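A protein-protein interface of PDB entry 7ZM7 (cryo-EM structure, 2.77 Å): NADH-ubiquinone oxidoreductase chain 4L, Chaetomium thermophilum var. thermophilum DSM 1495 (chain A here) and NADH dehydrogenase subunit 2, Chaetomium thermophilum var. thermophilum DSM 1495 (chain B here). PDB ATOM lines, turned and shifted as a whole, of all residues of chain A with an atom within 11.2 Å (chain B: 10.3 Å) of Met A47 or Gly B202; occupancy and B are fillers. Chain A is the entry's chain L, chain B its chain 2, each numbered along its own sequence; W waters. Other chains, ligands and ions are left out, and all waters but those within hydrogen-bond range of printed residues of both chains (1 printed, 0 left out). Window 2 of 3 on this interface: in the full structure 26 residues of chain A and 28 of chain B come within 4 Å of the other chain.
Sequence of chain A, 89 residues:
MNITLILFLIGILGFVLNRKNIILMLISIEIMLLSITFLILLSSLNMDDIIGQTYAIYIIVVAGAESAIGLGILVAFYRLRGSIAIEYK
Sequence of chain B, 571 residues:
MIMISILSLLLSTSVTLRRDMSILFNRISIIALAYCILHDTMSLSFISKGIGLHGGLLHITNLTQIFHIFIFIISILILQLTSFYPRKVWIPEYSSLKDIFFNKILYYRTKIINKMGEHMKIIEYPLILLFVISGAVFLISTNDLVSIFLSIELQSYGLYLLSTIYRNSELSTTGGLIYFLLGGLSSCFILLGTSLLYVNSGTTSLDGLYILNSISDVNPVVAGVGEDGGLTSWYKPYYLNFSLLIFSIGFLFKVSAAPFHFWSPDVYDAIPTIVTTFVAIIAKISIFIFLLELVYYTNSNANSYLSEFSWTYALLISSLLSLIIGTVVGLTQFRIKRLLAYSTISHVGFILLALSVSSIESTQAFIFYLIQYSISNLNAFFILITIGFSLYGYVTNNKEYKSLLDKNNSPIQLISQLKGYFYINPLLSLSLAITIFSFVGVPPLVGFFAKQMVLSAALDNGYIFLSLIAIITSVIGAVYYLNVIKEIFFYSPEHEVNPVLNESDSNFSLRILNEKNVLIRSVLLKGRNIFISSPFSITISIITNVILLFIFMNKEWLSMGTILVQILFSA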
ATOM      1  N   PHE A  38     -20.931   7.110 -21.769  1.00  0.00           N
ATOM      2  CA  PHE A  38     -21.825   8.105 -21.209  1.00  0.00           C
ATOM      3  C   PHE A  38     -22.920   7.471 -20.363  1.00  0.00           C
ATOM      4  O   PHE A  38     -23.310   8.027 -19.329  1.00  0.00           O
ATOM      5  CB  PHE A  38     -22.396   8.930 -22.345  1.00  0.00           C
ATOM      6  CG  PHE A  38     -23.038  10.182 -21.909  1.00  0.00           C
ATOM      7  CD1 PHE A  38     -22.377  11.064 -21.090  1.00  0.00           C
ATOM      8  CD2 PHE A  38     -24.337  10.453 -22.262  1.00  0.00           C
ATOM      9  CE1 PHE A  38     -22.994  12.206 -20.676  1.00  0.00           C
ATOM     10  CE2 PHE A  38     -24.936  11.589 -21.847  1.00  0.00           C
ATOM     11  CZ  PHE A  38     -24.266  12.449 -21.058  1.00  0.00           C
ATOM     12  N   LEU A  39     -23.430   6.310 -20.780  1.00  0.00           N
ATOM     13  CA  LEU A  39     -24.418   5.609 -19.972  1.00  0.00           C
ATOM     14  C   LEU A  39     -23.812   5.103 -18.668  1.00  0.00           C
ATOM     15  O   LEU A  39     -24.415   5.253 -17.602  1.00  0.00           O
ATOM     16  CB  LEU A  39     -25.030   4.461 -20.770  1.00  0.00           C
ATOM     17  CG  LEU A  39     -25.742   3.363 -19.980  1.00  0.00           C
ATOM     18  CD1 LEU A  39     -26.988   3.884 -19.336  1.00  0.00           C
ATOM     19  CD2 LEU A  39     -26.070   2.170 -20.839  1.00  0.00           C
ATOM     20  N   ILE A  40     -22.612   4.530 -18.723  1.00  0.00           N
ATOM     21  CA  ILE A  40     -21.954   4.067 -17.504  1.00  0.00           C
ATOM     22  C   ILE A  40     -21.781   5.211 -16.518  1.00  0.00           C
ATOM     23  O   ILE A  40     -21.996   5.046 -15.314  1.00  0.00           O
ATOM     24  CB  ILE A  40     -20.601   3.405 -17.841  1.00  0.00           C
ATOM     25  CG1 ILE A  40     -20.811   2.067 -18.523  1.00  0.00           C
ATOM     26  CG2 ILE A  40     -19.772   3.201 -16.606  1.00  0.00           C
ATOM     27  CD1 ILE A  40     -19.696   1.700 -19.391  1.00  0.00           C
ATOM     28  N   LEU A  41     -21.382   6.383 -17.014  1.00  0.00           N
ATOM     29  CA  LEU A  41     -21.121   7.535 -16.158  1.00  0.00           C
ATOM     30  C   LEU A  41     -22.377   8.047 -15.469  1.00  0.00           C
ATOM     31  O   LEU A  41     -22.341   8.392 -14.286  1.00  0.00           O
ATOM     32  CB  LEU A  41     -20.495   8.650 -16.977  1.00  0.00           C
ATOM     33  CG  LEU A  41     -19.037   8.460 -17.347  1.00  0.00           C
ATOM     34  CD1 LEU A  41     -18.640   9.546 -18.303  1.00  0.00           C
ATOM     35  CD2 LEU A  41     -18.205   8.488 -16.093  1.00  0.00           C
ATOM     36  N   LEU A  42     -23.485   8.144 -16.195  1.00  0.00           N
ATOM     37  CA  LEU A  42     -24.708   8.681 -15.608  1.00  0.00           C
ATOM     38  C   LEU A  42     -25.308   7.727 -14.594  1.00  0.00           C
ATOM     39  O   LEU A  42     -25.847   8.157 -13.575  1.00  0.00           O
ATOM     40  CB  LEU A  42     -25.714   9.013 -16.701  1.00  0.00           C
ATOM     41  CG  LEU A  42     -25.785  10.486 -17.071  1.00  0.00           C
ATOM     42  CD1 LEU A  42     -24.464  10.964 -17.591  1.00  0.00           C
ATOM     43  CD2 LEU A  42     -26.846  10.642 -18.108  1.00  0.00           C
ATOM     44  N   SER A  43     -25.070   6.436 -14.757  1.00  0.00           N
ATOM     45  CA  SER A  43     -25.554   5.465 -13.745  1.00  0.00           C
ATOM     46  C   SER A  43     -24.627   5.467 -12.532  1.00  0.00           C
ATOM     47  O   SER A  43     -25.109   5.227 -11.423  1.00  0.00           O
ATOM     48  CB  SER A  43     -25.680   4.112 -14.362  1.00  0.00           C
ATOM     49  OG  SER A  43     -26.354   4.203 -15.605  1.00  0.00           O
ATOM     50  N   SER A  44     -23.348   5.751 -12.735  1.00  0.00           N
ATOM     51  CA  SER A  44     -22.393   5.862 -11.601  1.00  0.00           C
ATOM     52  C   SER A  44     -22.769   7.028 -10.682  1.00  0.00           C
ATOM     53  O   SER A  44     -22.673   6.859  -9.467  1.00  0.00           O
ATOM     54  CB  SER A  44     -21.018   6.024 -12.146  1.00  0.00           C
ATOM     55  OG  SER A  44     -20.791   5.088 -13.177  1.00  0.00           O
ATOM     56  N   LEU A  45     -23.179   8.165 -11.243  1.00  0.00           N
ATOM     57  CA  LEU A  45     -23.636   9.328 -10.442  1.00  0.00           C
ATOM     58  C   LEU A  45     -24.863   8.902  -9.639  1.00  0.00           C
ATOM     59  O   LEU A  45     -24.959   9.274  -8.474  1.00  0.00           O
ATOM     60  CB  LEU A  45     -23.979  10.461 -11.415  1.00  0.00           C
ATOM     61  CG  LEU A  45     -24.326  11.799 -10.773  1.00  0.00           C
ATOM     62  CD1 LEU A  45     -23.123  12.362 -10.032  1.00  0.00           C
ATOM     63  CD2 LEU A  45     -24.825  12.783 -11.817  1.00  0.00           C
ATOM     64  N   ASN A  46     -25.747   8.123 -10.238  1.00  0.00           N
ATOM     65  CA  ASN A  46     -26.974   7.623  -9.562  1.00  0.00           C
ATOM     66  C   ASN A  46     -26.662   6.700  -8.391  1.00  0.00           C
ATOM     67  O   ASN A  46     -27.445   6.734  -7.439  1.00  0.00           O
ATOM     68  CB  ASN A  46     -27.914   6.908 -10.527  1.00  0.00           C
ATOM     69  CG  ASN A  46     -28.432   7.803 -11.629  1.00  0.00           C
ATOM     70  OD1 ASN A  46     -28.194   9.009 -11.628  1.00  0.00           O
ATOM     71  ND2 ASN A  46     -29.145   7.221 -12.576  1.00  0.00           N
ATOM     72  N   MET A  47     -25.573   5.925  -8.429  1.00  0.00           N
ATOM     73  CA  MET A  47     -25.353   4.884  -7.388  1.00  0.00           C
ATOM     74  C   MET A  47     -24.222   5.295  -6.441  1.00  0.00           C
ATOM     75  O   MET A  47     -23.920   4.510  -5.535  1.00  0.00           O
ATOM     76  CB  MET A  47     -25.052   3.526  -8.023  1.00  0.00           C
ATOM     77  CG  MET A  47     -26.017   3.094  -9.109  1.00  0.00           C
ATOM     78  SD  MET A  47     -25.488   1.545  -9.906  1.00  0.00           S
ATOM     79  CE  MET A  47     -23.748   1.873 -10.173  1.00  0.00           C
ATOM     80  N   ASP A  48     -23.645   6.486  -6.620  1.00  0.00           N
ATOM     81  CA  ASP A  48     -22.523   6.984  -5.774  1.00  0.00           C
ATOM     82  C   ASP A  48     -21.326   6.040  -5.868  1.00  0.00           C
ATOM     83  O   ASP A  48     -20.703   5.773  -4.827  1.00  0.00           O
ATOM     84  CB  ASP A  48     -22.940   7.195  -4.319  1.00  0.00           C
ATOM     85  CG  ASP A  48     -21.835   7.788  -3.464  1.00  0.00           C
ATOM     86  OD1 ASP A  48     -21.179   8.737  -3.937  1.00  0.00           O
ATOM     87  OD2 ASP A  48     -21.629   7.290  -2.337  1.00  0.00           O
ATOM     88  N   ASP A  49     -21.034   5.543  -7.065  1.00  0.00           N
ATOM     89  CA  ASP A  49     -19.920   4.575  -7.244  1.00  0.00           C
ATOM     90  C   ASP A  49     -18.799   5.206  -8.075  1.00  0.00           C
ATOM     91  O   ASP A  49     -19.094   5.798  -9.117  1.00  0.00           O
ATOM     92  CB  ASP A  49     -20.428   3.237  -7.783  1.00  0.00           C
ATOM     93  CG  ASP A  49     -19.559   2.057  -7.382  1.00  0.00           C
ATOM     94  OD1 ASP A  49     -18.551   2.284  -6.683  1.00  0.00           O
ATOM     95  OD2 ASP A  49     -19.899   0.917  -7.766  1.00  0.00           O
ATOM     96  N   ILE A  50     -17.557   5.046  -7.633  1.00  0.00           N
ATOM     97  CA  ILE A  50     -16.387   5.591  -8.372  1.00  0.00           C
ATOM     98  C   ILE A  50     -15.909   4.587  -9.425  1.00  0.00           C
ATOM     99  O   ILE A  50     -15.124   4.985 -10.288  1.00  0.00           O
ATOM    100  CB  ILE A  50     -15.278   5.943  -7.360  1.00  0.00           C
ATOM    101  CG1 ILE A  50     -14.357   7.057  -7.865  1.00  0.00           C
ATOM    102  CG2 ILE A  50     -14.508   4.709  -6.926  1.00  0.00           C
ATOM    103  CD1 ILE A  50     -15.050   8.385  -8.060  1.00  0.00           C
ATOM    104  N   ILE A  51     -16.354   3.329  -9.338  1.00  0.00           N
ATOM    105  CA  ILE A  51     -15.855   2.272 -10.266  1.00  0.00           C
ATOM    106  C   ILE A  51     -16.467   2.526 -11.639  1.00  0.00           C
ATOM    107  O   ILE A  51     -15.808   2.198 -12.639  1.00  0.00           O
ATOM    108  CB  ILE A  51     -16.121   0.852  -9.727  1.00  0.00           C
ATOM    109  CG1 ILE A  51     -14.900  -0.052  -9.898  1.00  0.00           C
ATOM    110  CG2 ILE A  51     -17.368   0.232 -10.337  1.00  0.00           C
ATOM    111  CD1 ILE A  51     -13.611   0.598  -9.466  1.00  0.00           C
ATOM    112  N   GLY A  52     -17.673   3.096 -11.681  1.00  0.00           N
ATOM    113  CA  GLY A  52     -18.226   3.455 -12.969  1.00  0.00           C
ATOM    114  C   GLY A  52     -17.433   4.550 -13.644  1.00  0.00           C
ATOM    115  O   GLY A  52     -17.286   4.560 -14.864  1.00  0.00           O
ATOM    116  N   GLN A  53     -16.920   5.491 -12.856  1.00  0.00           N
ATOM    117  CA  GLN A  53     -16.064   6.540 -13.389  1.00  0.00           C
ATOM    118  C   GLN A  53     -14.772   5.974 -13.942  1.00  0.00           C
ATOM    119  O   GLN A  53     -14.287   6.414 -14.984  1.00  0.00           O
ATOM    120  CB  GLN A  53     -15.760   7.550 -12.295  1.00  0.00           C
ATOM    121  CG  GLN A  53     -16.942   8.320 -11.843  1.00  0.00           C
ATOM    122  CD  GLN A  53     -16.607   9.752 -11.612  1.00  0.00           C
ATOM    123  OE1 GLN A  53     -15.816  10.326 -12.336  1.00  0.00           O
ATOM    124  NE2 GLN A  53     -17.199  10.338 -10.598  1.00  0.00           N
ATOM    125  N   THR A  54     -14.180   5.029 -13.223  1.00  0.00           N
ATOM    126  CA  THR A  54     -12.916   4.439 -13.629  1.00  0.00           C
ATOM    127  C   THR A  54     -13.079   3.599 -14.885  1.00  0.00           C
ATOM    128  O   THR A  54     -12.260   3.663 -15.801  1.00  0.00           O
ATOM    129  CB  THR A  54     -12.389   3.596 -12.484  1.00  0.00           C
ATOM    130  OG1 THR A  54     -12.206   4.436 -11.347  1.00  0.00           O
ATOM    131  CG2 THR A  54     -11.082   2.943 -12.872  1.00  0.00           C
ATOM    132  N   TYR A  55     -14.155   2.829 -14.944  1.00  0.00           N
ATOM    133  CA  TYR A  55     -14.463   2.026 -16.113  1.00  0.00           C
ATOM    134  C   TYR A  55     -14.658   2.907 -17.344  1.00  0.00           C
ATOM    135  O   TYR A  55     -14.251   2.541 -18.447  1.00  0.00           O
ATOM    136  CB  TYR A  55     -15.683   1.182 -15.759  1.00  0.00           C
ATOM    137  CG  TYR A  55     -16.374   0.359 -16.796  1.00  0.00           C
ATOM    138  CD1 TYR A  55     -15.677  -0.321 -17.770  1.00  0.00           C
ATOM    139  CD2 TYR A  55     -17.720   0.099 -16.664  1.00  0.00           C
ATOM    140  CE1 TYR A  55     -16.331  -1.132 -18.661  1.00  0.00           C
ATOM    141  CE2 TYR A  55     -18.378  -0.722 -17.532  1.00  0.00           C
ATOM    142  CZ  TYR A  55     -17.690  -1.325 -18.530  1.00  0.00           C
ATOM    143  OH  TYR A  55     -18.382  -2.131 -19.394  1.00  0.00           O
ATOM    144  N   ASP B 144     -13.874 -10.137 -13.796  1.00  0.00           N
ATOM    145  CA  ASP B 144     -14.585  -8.833 -13.768  1.00  0.00           C
ATOM    146  C   ASP B 144     -14.960  -8.400 -15.191  1.00  0.00           C
ATOM    147  O   ASP B 144     -14.306  -8.860 -16.125  1.00  0.00           O
ATOM    148  CB  ASP B 144     -13.710  -7.800 -13.059  1.00  0.00           C
ATOM    149  CG  ASP B 144     -14.461  -6.576 -12.584  1.00  0.00           C
ATOM    150  OD1 ASP B 144     -14.715  -5.687 -13.419  1.00  0.00           O
ATOM    151  OD2 ASP B 144     -14.777  -6.522 -11.383  1.00  0.00           O
ATOM    152  N   LEU B 145     -15.988  -7.554 -15.337  1.00  0.00           N
ATOM    153  CA  LEU B 145     -16.398  -7.065 -16.673  1.00  0.00           C
ATOM    154  C   LEU B 145     -15.244  -6.255 -17.249  1.00  0.00           C
ATOM    155  O   LEU B 145     -14.939  -6.470 -18.426  1.00  0.00           O
ATOM    156  CB  LEU B 145     -17.658  -6.215 -16.501  1.00  0.00           C
ATOM    157  CG  LEU B 145     -18.888  -6.983 -16.016  1.00  0.00           C
ATOM    158  CD1 LEU B 145     -20.056  -6.045 -15.771  1.00  0.00           C
ATOM    159  CD2 LEU B 145     -19.271  -8.079 -16.992  1.00  0.00           C
ATOM    160  N   THR B 194     -21.649  -5.505 -21.387  1.00  0.00           N
ATOM    161  CA  THR B 194     -21.099  -5.373 -20.045  1.00  0.00           C
ATOM    162  C   THR B 194     -21.612  -4.120 -19.358  1.00  0.00           C
ATOM    163  O   THR B 194     -21.892  -4.136 -18.161  1.00  0.00           O
ATOM    164  CB  THR B 194     -19.580  -5.351 -20.116  1.00  0.00           C
ATOM    165  OG1 THR B 194     -19.173  -4.371 -21.066  1.00  0.00           O
ATOM    166  CG2 THR B 194     -19.053  -6.682 -20.538  1.00  0.00           C
ATOM    167  N   SER B 195     -21.741  -3.025 -20.103  1.00  0.00           N
ATOM    168  CA  SER B 195     -22.251  -1.790 -19.527  1.00  0.00           C
ATOM    169  C   SER B 195     -23.663  -1.975 -18.986  1.00  0.00           C
ATOM    170  O   SER B 195     -23.976  -1.528 -17.882  1.00  0.00           O
ATOM    171  CB  SER B 195     -22.227  -0.686 -20.575  1.00  0.00           C
ATOM    172  OG  SER B 195     -23.315  -0.822 -21.464  1.00  0.00           O
ATOM    173  N   LEU B 196     -24.529  -2.630 -19.755  1.00  0.00           N
ATOM    174  CA  LEU B 196     -25.889  -2.875 -19.309  1.00  0.00           C
ATOM    175  C   LEU B 196     -25.954  -3.861 -18.166  1.00  0.00           C
ATOM    176  O   LEU B 196     -26.970  -3.923 -17.473  1.00  0.00           O
ATOM    177  CB  LEU B 196     -26.737  -3.381 -20.464  1.00  0.00           C
ATOM    178  CG  LEU B 196     -27.204  -2.314 -21.430  1.00  0.00           C
ATOM    179  CD1 LEU B 196     -27.741  -3.029 -22.590  1.00  0.00           C
ATOM    180  CD2 LEU B 196     -28.254  -1.482 -20.790  1.00  0.00           C
ATOM    181  N   LEU B 197     -24.900  -4.634 -17.959  1.00  0.00           N
ATOM    182  CA  LEU B 197     -24.835  -5.487 -16.786  1.00  0.00           C
ATOM    183  C   LEU B 197     -24.595  -4.675 -15.528  1.00  0.00           C
ATOM    184  O   LEU B 197     -25.339  -4.802 -14.555  1.00  0.00           O
ATOM    185  CB  LEU B 197     -23.737  -6.525 -16.969  1.00  0.00           C
ATOM    186  CG  LEU B 197     -24.158  -7.777 -17.711  1.00  0.00           C
ATOM    187  CD1 LEU B 197     -22.931  -8.499 -18.182  1.00  0.00           C
ATOM    188  CD2 LEU B 197     -24.986  -8.648 -16.815  1.00  0.00           C
ATOM    189  N   TYR B 198     -23.550  -3.849 -15.529  1.00  0.00           N
ATOM    190  CA  TYR B 198     -23.188  -3.074 -14.347  1.00  0.00           C
ATOM    191  C   TYR B 198     -24.268  -2.057 -14.004  1.00  0.00           C
ATOM    192  O   TYR B 198     -24.628  -1.883 -12.840  1.00  0.00           O
ATOM    193  CB  TYR B 198     -21.824  -2.404 -14.587  1.00  0.00           C
ATOM    194  CG  TYR B 198     -21.531  -1.220 -13.713  1.00  0.00           C
ATOM    195  CD1 TYR B 198     -21.079  -1.388 -12.412  1.00  0.00           C
ATOM    196  CD2 TYR B 198     -21.714   0.064 -14.183  1.00  0.00           C
ATOM    197  CE1 TYR B 198     -20.826  -0.325 -11.609  1.00  0.00           C
ATOM    198  CE2 TYR B 198     -21.465   1.147 -13.378  1.00  0.00           C
ATOM    199  CZ  TYR B 198     -21.017   0.944 -12.093  1.00  0.00           C
ATOM    200  OH  TYR B 198     -20.759   2.024 -11.297  1.00  0.00           O
ATOM    201  N   VAL B 199     -24.865  -1.461 -15.023  1.00  0.00           N
ATOM    202  CA  VAL B 199     -25.871  -0.376 -14.846  1.00  0.00           C
ATOM    203  C   VAL B 199     -27.181  -0.897 -14.233  1.00  0.00           C
ATOM    204  O   VAL B 199     -27.982  -0.088 -13.766  1.00  0.00           O
ATOM    205  CB  VAL B 199     -26.019   0.343 -16.203  1.00  0.00           C
ATOM    206  CG1 VAL B 199     -27.404   0.796 -16.590  1.00  0.00           C
ATOM    207  CG2 VAL B 199     -24.953   1.395 -16.448  1.00  0.00           C
ATOM    208  N   ASN B 200     -27.370  -2.213 -14.197  1.00  0.00           N
ATOM    209  CA  ASN B 200     -28.614  -2.788 -13.634  1.00  0.00           C
ATOM    210  C   ASN B 200     -28.313  -3.543 -12.353  1.00  0.00           C
ATOM    211  O   ASN B 200     -29.223  -3.695 -11.549  1.00  0.00           O
ATOM    212  CB  ASN B 200     -29.285  -3.710 -14.638  1.00  0.00           C
ATOM    213  CG  ASN B 200     -30.054  -2.973 -15.715  1.00  0.00           C
ATOM    214  OD1 ASN B 200     -31.036  -2.299 -15.429  1.00  0.00           O
ATOM    215  ND2 ASN B 200     -29.632  -3.113 -16.958  1.00  0.00           N
ATOM    216  N   SER B 201     -27.071  -3.966 -12.164  1.00  0.00           N
ATOM    217  CA  SER B 201     -26.677  -4.788 -11.000  1.00  0.00           C
ATOM    218  C   SER B 201     -25.778  -4.027 -10.031  1.00  0.00           C
ATOM    219  O   SER B 201     -25.549  -4.557  -8.951  1.00  0.00           O
ATOM    220  CB  SER B 201     -25.977  -5.971 -11.527  1.00  0.00           C
ATOM    221  OG  SER B 201     -24.790  -5.588 -12.189  1.00  0.00           O
ATOM    222  N   GLY B 202     -25.221  -2.881 -10.418  1.00  0.00           N
ATOM    223  CA  GLY B 202     -24.289  -2.193  -9.553  1.00  0.00           C
ATOM    224  C   GLY B 202     -22.965  -2.874  -9.319  1.00  0.00           C
ATOM    225  O   GLY B 202     -22.178  -2.393  -8.512  1.00  0.00           O
ATOM    226  N   THR B 203     -22.707  -3.971 -10.025  1.00  0.00           N
ATOM    227  CA  THR B 203     -21.474  -4.755  -9.789  1.00  0.00           C
ATOM    228  C   THR B 203     -20.752  -5.035 -11.100  1.00  0.00           C
ATOM    229  O   THR B 203     -21.429  -5.064 -12.132  1.00  0.00           O
ATOM    230  CB  THR B 203     -21.781  -6.094  -9.102  1.00  0.00           C
ATOM    231  OG1 THR B 203     -20.541  -6.753  -8.837  1.00  0.00           O
ATOM    232  CG2 THR B 203     -22.691  -7.005  -9.893  1.00  0.00           C
ATOM    233  N   THR B 204     -19.425  -5.166 -11.062  1.00  0.00           N
ATOM    234  CA  THR B 204     -18.669  -5.580 -12.269  1.00  0.00           C
ATOM    235  C   THR B 204     -18.124  -6.997 -12.051  1.00  0.00           C
ATOM    236  O   THR B 204     -17.640  -7.586 -13.021  1.00  0.00           O
ATOM    237  CB  THR B 204     -17.594  -4.553 -12.631  1.00  0.00           C
ATOM    238  OG1 THR B 204     -16.779  -4.301 -11.491  1.00  0.00           O
ATOM    239  CG2 THR B 204     -18.162  -3.244 -13.129  1.00  0.00           C
ATOM    240  N   SER B 205     -18.226  -7.517 -10.824  1.00  0.00           N
ATOM    241  CA  SER B 205     -17.743  -8.878 -10.473  1.00  0.00           C
ATOM    242  C   SER B 205     -18.686  -9.957 -11.010  1.00  0.00           C
ATOM    243  O   SER B 205     -19.895  -9.848 -10.778  1.00  0.00           O
ATOM    244  CB  SER B 205     -17.603  -9.004  -8.984  1.00  0.00           C
ATOM    245  OG  SER B 205     -18.863  -8.938  -8.340  1.00  0.00           O
ATOM    246  N   LEU B 206     -18.145 -10.963 -11.693  1.00  0.00           N
ATOM    247  CA  LEU B 206     -18.957 -12.063 -12.268  1.00  0.00           C
ATOM    248  C   LEU B 206     -19.630 -12.877 -11.161  1.00  0.00           C
ATOM    249  O   LEU B 206     -20.796 -13.227 -11.336  1.00  0.00           O
ATOM    250  CB  LEU B 206     -18.053 -12.942 -13.133  1.00  0.00           C
ATOM    251  CG  LEU B 206     -17.636 -12.334 -14.468  1.00  0.00           C
ATOM    252  CD1 LEU B 206     -16.914 -13.364 -15.323  1.00  0.00           C
ATOM    253  CD2 LEU B 206     -18.845 -11.784 -15.206  1.00  0.00           C
ATOM    254  N   GLY B 208     -20.684 -11.931  -8.167  1.00  0.00           N
ATOM    255  CA  GLY B 208     -21.890 -11.229  -7.690  1.00  0.00           C
ATOM    256  C   GLY B 208     -23.050 -11.375  -8.656  1.00  0.00           C
ATOM    257  O   GLY B 208     -24.159 -11.613  -8.179  1.00  0.00           O
ATOM    258  N   LEU B 209     -22.799 -11.257  -9.959  1.00  0.00           N
ATOM    259  CA  LEU B 209     -23.831 -11.450 -11.004  1.00  0.00           C
ATOM    260  C   LEU B 209     -24.336 -12.889 -10.967  1.00  0.00           C
ATOM    261  O   LEU B 209     -25.541 -13.082 -11.164  1.00  0.00           O
ATOM    262  CB  LEU B 209     -23.186 -11.154 -12.356  1.00  0.00           C
ATOM    263  CG  LEU B 209     -23.115  -9.678 -12.741  1.00  0.00           C
ATOM    264  CD1 LEU B 209     -22.194  -9.473 -13.933  1.00  0.00           C
ATOM    265  CD2 LEU B 209     -24.501  -9.132 -13.038  1.00  0.00           C
ATOM    266  N   LEU B 212     -26.668 -13.080  -7.971  1.00  0.00           N
ATOM    267  CA  LEU B 212     -27.935 -12.361  -8.259  1.00  0.00           C
ATOM    268  C   LEU B 212     -28.783 -13.239  -9.178  1.00  0.00           C
ATOM    269  O   LEU B 212     -30.002 -13.233  -9.013  1.00  0.00           O
ATOM    270  CB  LEU B 212     -27.617 -11.002  -8.891  1.00  0.00           C
ATOM    271  CG  LEU B 212     -27.043  -9.941  -7.959  1.00  0.00           C
ATOM    272  CD1 LEU B 212     -26.656  -8.698  -8.745  1.00  0.00           C
ATOM    273  CD2 LEU B 212     -28.035  -9.592  -6.866  1.00  0.00           C
ATOM    274  N   TYR B 239     -32.560  -8.397 -17.290  1.00  0.00           N
ATOM    275  CA  TYR B 239     -31.342  -7.826 -17.891  1.00  0.00           C
ATOM    276  C   TYR B 239     -30.271  -8.883 -18.090  1.00  0.00           C
ATOM    277  O   TYR B 239     -29.594  -8.770 -19.092  1.00  0.00           O
ATOM    278  CB  TYR B 239     -30.811  -6.693 -17.010  1.00  0.00           C
ATOM    279  CG  TYR B 239     -30.232  -7.091 -15.677  1.00  0.00           C
ATOM    280  CD1 TYR B 239     -31.047  -7.317 -14.583  1.00  0.00           C
ATOM    281  CD2 TYR B 239     -28.864  -7.217 -15.504  1.00  0.00           C
ATOM    282  CE1 TYR B 239     -30.520  -7.682 -13.357  1.00  0.00           C
ATOM    283  CE2 TYR B 239     -28.321  -7.587 -14.286  1.00  0.00           C
ATOM    284  CZ  TYR B 239     -29.154  -7.815 -13.209  1.00  0.00           C
ATOM    285  OH  TYR B 239     -28.632  -8.174 -12.002  1.00  0.00           O
HETATM  286  O   HOH W   1     -27.711   2.324 -12.672  1.00  0.00           O
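The side-chain hydroxyl (OG1) of Thr B194 sits at hydrogen-bond distance from the side-chain hydroxyl (OH) of Tyr A55 (2.9 Å). N of Gly A52 sits at hydrogen-bond distance from OH of Tyr B198.
The backbone carbonyl oxygen of Leu A39 sits at hydrogen-bond distance from the side-chain hydroxyl of Ser A43, at 3.0 Å. The side-chain hydroxyl (OG) of Ser A44 lies within hydrogen-bond range of the backbone carbonyl oxygen (O) of Ile A40 (2.5 Å). The backbone NH of Asp A49 is in hydrogen-bond range of the backbone carbonyl oxygen of Ser A44, at 3.2 Å.
CB of Ser B195 touches CD1 of Ile A40, 3.7 Å away. Ser A43 touches Val B199. OG of Ser A44 touches OH of Tyr B198, at 3.6 Å. Met A47 touches Tyr B198. SD of Met A47 touches CA of Gly B202, at 3.9 Å. Tyr B198 touches Asp A49 (OH to CB, 3.7 Å). Ile A51 touches Tyr B198 (CG2 to CE1, 3.7 Å). Tyr A55 touches Ser B195.
Of the printed residues of chain B, Ile A40 touches Ser B195. Printed residues of chain B within 4 Å of Ser A43: Val B199. Of chain B, only Tyr B198 (3.6 Å) comes within 4 Å of Ser A44. No residue of chain B comes within 4 Å of Asn A46. Met A47 touches just these residues of chain B: Tyr B198 (3.2 Å) and Gly B202 (3.9 Å). No residue of chain B comes within 4 Å of Asp A48. Ile A50 touches none of the printed residues of chain B. Of the printed residues of chain B, Ile A51 touches Tyr B198 (3.7 Å). Of the printed residues of chain B, Gly A52 touches Tyr B198 (3.3 Å). Of the printed residues of chain B, Tyr A55 touches Thr B194 (2.9 Å) and Ser B195 (3.5 Å). No residue of chain A comes within 4 Å of Ser B201. Of the printed residues of chain A, Gly B202 touches Met A47 (3.9 Å). Thr B203 touches none of the printed residues of chain A. The nearest residue of chain A that does not touch Gly B202 is Asp A49 (4.1 Å).
Of the 19 printed residues of chain B, 5 touch a printed residue of chain A. Hydrophobic or aromatic side chains of chain B within 4 Å of the printed part of chain A: Tyr B198 and Val B199. Of the 18 printed residues of chain A, 8 touch a printed residue of chain B. Printed residues of chain A that touch a printed residue of chain B: Ile A40, Ser A43, Ser A44, Met A47, Asp A49, Ile A51, Gly A52 and Tyr A55. Hydrophobic or aromatic side chains of chain A within 4 Å of the printed part of chain B: Ile A40, Met A47, Ile A51 and Tyr A55. Among the printed residues, no Asp or Glu carboxylate lies within 4 Å of a Lys or Arg side-chain nitrogen of the other chain.
Water W1 bridges O of Val B199 and SD of Met A47.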
